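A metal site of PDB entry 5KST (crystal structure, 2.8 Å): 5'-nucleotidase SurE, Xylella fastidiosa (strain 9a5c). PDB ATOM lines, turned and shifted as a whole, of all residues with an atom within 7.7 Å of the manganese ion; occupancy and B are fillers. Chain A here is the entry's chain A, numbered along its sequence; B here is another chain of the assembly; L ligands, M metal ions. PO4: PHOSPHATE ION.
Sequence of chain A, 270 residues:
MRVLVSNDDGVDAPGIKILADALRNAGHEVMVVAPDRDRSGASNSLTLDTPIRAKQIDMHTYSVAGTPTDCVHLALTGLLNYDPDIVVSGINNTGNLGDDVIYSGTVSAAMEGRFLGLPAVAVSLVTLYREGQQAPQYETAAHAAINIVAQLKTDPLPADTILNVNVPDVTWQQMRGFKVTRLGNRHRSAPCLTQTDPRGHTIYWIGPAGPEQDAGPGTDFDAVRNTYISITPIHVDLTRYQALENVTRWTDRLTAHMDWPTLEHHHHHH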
ATOM      1  N   ASN A   7       3.338  19.387  22.184  1.00  0.00           N
ATOM      2  CA  ASN A   7       3.211  20.783  22.596  1.00  0.00           C
ATOM      3  C   ASN A   7       2.962  21.639  21.356  1.00  0.00           C
ATOM      4  O   ASN A   7       2.632  21.112  20.293  1.00  0.00           O
ATOM      5  CB  ASN A   7       4.460  21.259  23.349  1.00  0.00           C
ATOM      6  CG  ASN A   7       5.678  21.412  22.463  1.00  0.00           C
ATOM      7  OD1 ASN A   7       5.719  20.908  21.332  1.00  0.00           O
ATOM      8  ND2 ASN A   7       6.690  22.096  22.970  1.00  0.00           N
ATOM      9  N   ASP A   8       3.118  22.949  21.485  1.00  0.00           N
ATOM     10  CA  ASP A   8       3.055  23.824  20.317  1.00  0.00           C
ATOM     11  C   ASP A   8       4.288  24.725  20.215  1.00  0.00           C
ATOM     12  O   ASP A   8       4.496  25.384  19.201  1.00  0.00           O
ATOM     13  CB  ASP A   8       1.788  24.663  20.338  1.00  0.00           C
ATOM     14  CG  ASP A   8       1.809  25.734  21.400  1.00  0.00           C
ATOM     15  OD1 ASP A   8       2.531  25.565  22.415  1.00  0.00           O
ATOM     16  OD2 ASP A   8       1.093  26.741  21.212  1.00  0.00           O
ATOM     17  N   ASP A   9       5.095  24.728  21.274  1.00  0.00           N
ATOM     18  CA  ASP A   9       6.313  25.527  21.325  1.00  0.00           C
ATOM     19  C   ASP A   9       7.448  24.879  20.533  1.00  0.00           C
ATOM     20  O   ASP A   9       8.486  25.503  20.309  1.00  0.00           O
ATOM     21  CB  ASP A   9       6.753  25.737  22.764  1.00  0.00           C
ATOM     22  CG  ASP A   9       5.656  26.312  23.618  1.00  0.00           C
ATOM     23  OD1 ASP A   9       4.788  27.013  23.069  1.00  0.00           O
ATOM     24  OD2 ASP A   9       5.669  26.082  24.836  1.00  0.00           O
ATOM     25  N   GLY A  10       7.244  23.637  20.127  1.00  0.00           N
ATOM     26  CA  GLY A  10       8.214  22.943  19.305  1.00  0.00           C
ATOM     27  C   GLY A  10       8.854  21.757  19.993  1.00  0.00           C
ATOM     28  O   GLY A  10       8.940  21.704  21.208  1.00  0.00           O
ATOM     29  N   ASP A  38       8.145  26.435  16.753  1.00  0.00           N
ATOM     30  CA  ASP A  38       7.171  27.060  17.624  1.00  0.00           C
ATOM     31  C   ASP A  38       5.958  27.517  16.806  1.00  0.00           C
ATOM     32  O   ASP A  38       6.096  28.306  15.877  1.00  0.00           O
ATOM     33  CB  ASP A  38       7.781  28.250  18.377  1.00  0.00           C
ATOM     34  CG  ASP A  38       6.947  28.677  19.574  1.00  0.00           C
ATOM     35  OD1 ASP A  38       5.710  28.524  19.540  1.00  0.00           O
ATOM     36  OD2 ASP A  38       7.545  29.175  20.559  1.00  0.00           O
ATOM     37  N   ARG A  39       4.791  27.004  17.169  1.00  0.00           N
ATOM     38  CA  ARG A  39       3.564  27.367  16.475  1.00  0.00           C
ATOM     39  C   ARG A  39       2.552  27.949  17.461  1.00  0.00           C
ATOM     40  O   ARG A  39       1.355  27.698  17.345  1.00  0.00           O
ATOM     41  CB  ARG A  39       2.977  26.151  15.747  1.00  0.00           C
ATOM     42  CG  ARG A  39       3.861  25.676  14.594  1.00  0.00           C
ATOM     43  CD  ARG A  39       3.383  24.407  13.892  1.00  0.00           C
ATOM     44  NE  ARG A  39       2.806  24.706  12.608  1.00  0.00           N
ATOM     45  CZ  ARG A  39       3.218  24.453  11.371  1.00  0.00           C
ATOM     46  NH1 ARG A  39       4.312  23.790  11.017  1.00  0.00           N
ATOM     47  NH2 ARG A  39       2.408  24.909  10.434  1.00  0.00           N
ATOM     48  N   SER A  40       3.046  28.734  18.413  1.00  0.00           N
ATOM     49  CA  SER A  40       2.196  29.285  19.472  1.00  0.00           C
ATOM     50  C   SER A  40       1.225  30.327  18.934  1.00  0.00           C
ATOM     51  O   SER A  40       0.208  30.625  19.565  1.00  0.00           O
ATOM     52  CB  SER A  40       3.056  29.908  20.581  1.00  0.00           C
ATOM     53  OG  SER A  40       3.840  28.919  21.229  1.00  0.00           O
ATOM     54  N   GLY A  41       1.526  30.884  17.761  1.00  0.00           N
ATOM     55  CA  GLY A  41       0.656  31.860  17.138  1.00  0.00           C
ATOM     56  C   GLY A  41       0.124  31.382  15.803  1.00  0.00           C
ATOM     57  O   GLY A  41      -0.167  32.183  14.915  1.00  0.00           O
ATOM     58  N   ILE A  91       5.339  21.196  28.139  1.00  0.00           N
ATOM     59  CA  ILE A  91       4.838  22.252  29.014  1.00  0.00           C
ATOM     60  C   ILE A  91       4.955  23.588  28.307  1.00  0.00           C
ATOM     61  O   ILE A  91       6.041  23.975  27.886  1.00  0.00           O
ATOM     62  CB  ILE A  91       5.595  22.282  30.335  1.00  0.00           C
ATOM     63  CG1 ILE A  91       5.504  20.910  31.010  1.00  0.00           C
ATOM     64  CG2 ILE A  91       5.047  23.393  31.228  1.00  0.00           C
ATOM     65  CD1 ILE A  91       6.469  20.727  32.159  1.00  0.00           C
ATOM     66  N   ASN A  92       3.828  24.270  28.150  1.00  0.00           N
ATOM     67  CA  ASN A  92       3.819  25.557  27.462  1.00  0.00           C
ATOM     68  C   ASN A  92       4.653  26.590  28.214  1.00  0.00           C
ATOM     69  O   ASN A  92       4.624  26.648  29.442  1.00  0.00           O
ATOM     70  CB  ASN A  92       2.381  26.044  27.278  1.00  0.00           C
ATOM     71  CG  ASN A  92       2.280  27.160  26.267  1.00  0.00           C
ATOM     72  OD1 ASN A  92       2.460  26.942  25.070  1.00  0.00           O
ATOM     73  ND2 ASN A  92       1.973  28.361  26.730  1.00  0.00           N
ATOM     74  N   ASN A  93       5.405  27.404  27.471  1.00  0.00           N
ATOM     75  CA  ASN A  93       6.277  28.393  28.077  1.00  0.00           C
ATOM     76  C   ASN A  93       5.483  29.519  28.742  1.00  0.00           C
ATOM     77  O   ASN A  93       6.000  30.235  29.600  1.00  0.00           O
ATOM     78  CB  ASN A  93       7.230  28.980  27.035  1.00  0.00           C
ATOM     79  CG  ASN A  93       6.518  29.384  25.752  1.00  0.00           C
ATOM     80  OD1 ASN A  93       5.283  29.419  25.705  1.00  0.00           O
ATOM     81  ND2 ASN A  93       7.291  29.696  24.716  1.00  0.00           N
ATOM     82  N   THR A  94       4.236  29.666  28.338  1.00  0.00           N
ATOM     83  CA  THR A  94       3.342  30.643  28.940  1.00  0.00           C
ATOM     84  C   THR A  94       2.067  29.964  29.449  1.00  0.00           C
ATOM     85  O   THR A  94       1.747  28.834  29.073  1.00  0.00           O
ATOM     86  CB  THR A  94       2.968  31.783  27.944  1.00  0.00           C
ATOM     87  OG1 THR A  94       2.021  31.290  26.987  1.00  0.00           O
ATOM     88  CG2 THR A  94       4.196  32.286  27.219  1.00  0.00           C
ATOM     89  N   GLY A  95       1.337  30.660  30.306  1.00  0.00           N
ATOM     90  CA  GLY A  95       0.086  30.134  30.822  1.00  0.00           C
ATOM     91  C   GLY A  95      -0.966  30.101  29.734  1.00  0.00           C
ATOM     92  O   GLY A  95      -0.926  30.881  28.783  1.00  0.00           O
ATOM     93  N   ASN A  96      -1.908  29.177  29.881  1.00  0.00           N
ATOM     94  CA  ASN A  96      -3.082  29.119  29.013  1.00  0.00           C
ATOM     95  C   ASN A  96      -4.346  29.154  29.843  1.00  0.00           C
ATOM     96  O   ASN A  96      -4.853  28.115  30.254  1.00  0.00           O
ATOM     97  CB  ASN A  96      -3.036  27.876  28.134  1.00  0.00           C
ATOM     98  CG  ASN A  96      -2.081  28.011  26.974  1.00  0.00           C
ATOM     99  OD1 ASN A  96      -1.127  27.254  26.853  1.00  0.00           O
ATOM    100  ND2 ASN A  96      -2.323  28.994  26.129  1.00  0.00           N
ATOM    101  N   SER A 104      -5.523  28.036  22.407  1.00  0.00           N
ATOM    102  CA  SER A 104      -4.188  27.578  22.769  1.00  0.00           C
ATOM    103  C   SER A 104      -3.714  26.402  21.909  1.00  0.00           C
ATOM    104  O   SER A 104      -4.431  25.420  21.740  1.00  0.00           O
ATOM    105  CB  SER A 104      -4.147  27.196  24.242  1.00  0.00           C
ATOM    106  OG  SER A 104      -2.954  26.484  24.549  1.00  0.00           O
ATOM    107  N   GLY A 105      -2.497  26.511  21.384  1.00  0.00           N
ATOM    108  CA  GLY A 105      -1.900  25.410  20.649  1.00  0.00           C
ATOM    109  C   GLY A 105      -1.674  24.208  21.554  1.00  0.00           C
ATOM    110  O   GLY A 105      -1.972  23.074  21.168  1.00  0.00           O
ATOM    111  N   THR A 106      -1.147  24.467  22.746  1.00  0.00           N
ATOM    112  CA  THR A 106      -0.930  23.428  23.748  1.00  0.00           C
ATOM    113  C   THR A 106      -2.212  22.647  23.971  1.00  0.00           C
ATOM    114  O   THR A 106      -2.234  21.429  23.868  1.00  0.00           O
ATOM    115  CB  THR A 106      -0.470  24.020  25.099  1.00  0.00           C
ATOM    116  OG1 THR A 106       0.742  24.764  24.903  1.00  0.00           O
ATOM    117  CG2 THR A 106      -0.228  22.914  26.116  1.00  0.00           C
ATOM    118  N   SER A 124       0.590  24.024  31.174  1.00  0.00           N
ATOM    119  CA  SER A 124       1.195  25.306  30.848  1.00  0.00           C
ATOM    120  C   SER A 124       1.858  25.924  32.080  1.00  0.00           C
ATOM    121  O   SER A 124       1.327  25.848  33.178  1.00  0.00           O
ATOM    122  CB  SER A 124       0.141  26.255  30.274  1.00  0.00           C
ATOM    123  OG  SER A 124      -0.601  25.607  29.258  1.00  0.00           O
ATOM    124  N   ARG B  37      11.363  32.645  17.369  1.00  0.00           N
ATOM    125  CA  ARG B  37      10.969  31.322  16.910  1.00  0.00           C
ATOM    126  C   ARG B  37      11.609  31.019  15.565  1.00  0.00           C
ATOM    127  O   ARG B  37      12.315  31.857  14.999  1.00  0.00           O
ATOM    128  CB  ARG B  37       9.448  31.213  16.818  1.00  0.00           C
ATOM    129  CG  ARG B  37       8.807  32.199  15.848  1.00  0.00           C
ATOM    130  CD  ARG B  37       7.294  32.096  15.896  1.00  0.00           C
ATOM    131  NE  ARG B  37       6.762  32.487  17.197  1.00  0.00           N
ATOM    132  CZ  ARG B  37       5.474  32.410  17.533  1.00  0.00           C
ATOM    133  NH1 ARG B  37       4.585  31.938  16.665  1.00  0.00           N
ATOM    134  NH2 ARG B  37       5.076  32.790  18.743  1.00  0.00           N
HETATM  135  P   PO4 L   1      -0.225  28.454  23.467  1.00  0.00           P
HETATM  136  O1  PO4 L   1      -0.367  27.001  23.853  1.00  0.00           O
HETATM  137  O2  PO4 L   1       1.192  28.710  23.004  1.00  0.00           O
HETATM  138  O3  PO4 L   1      -1.179  28.773  22.331  1.00  0.00           O
HETATM  139  O4  PO4 L   1      -0.509  29.344  24.647  1.00  0.00           O
HETATM  140 MN    MN M   1       3.026  27.786  23.131  1.00  0.00          MN
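OD1 of Asn 93 touches the manganese ion (3.8 Å).
Five residues have an atom within 4 Å of the manganese ion: Asp 8, Asp 9, Ser 40, Asn 92 and Asn 93.
The manganese ion is bound by the side-chain carboxylate (OD1) of Asp 9 (1.9 Å).
O2 of the ligand is bound to the manganese ion, 2.1 Å away.
The manganese ion is bound by OD1 of Asn 92 (2.2 Å).
OG of Ser 40 binds the manganese ion, at 2.4 Å.
OD1 of Asp 8 is bound to the manganese ion (2.4 Å).
Slightly farther from the manganese ion lies OD2 of Asp 8 (2.9 Å).
OD2 of Asp 9 lies within hydrogen-bond range of N of Asn 93, 3.0 Å away.
The side-chain amide oxygen (OD1) of Asn 92 sits close to the side-chain hydroxyl (OG1) of Thr 106, at 2.8 Å.
The side-chain amide nitrogen (ND2) of Asn 92 sits at hydrogen-bond distance from the backbone carbonyl oxygen (O) of Thr 94, 2.4 Å away.
The side-chain amide oxygen of Asn 96 lies within hydrogen-bond range of the side-chain amide nitrogen of Asn 92, 3.3 Å away.
The backbone NH of Ser 40 lies within hydrogen-bond range of the side-chain carboxylate of Asp 38, at 2.9 Å.
OD1 of Asp 8 sits close to OG1 of Thr 106 (3.2 Å).
O of Asp 8 sits at hydrogen-bond distance from N of Arg 39, at 2.6 Å.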
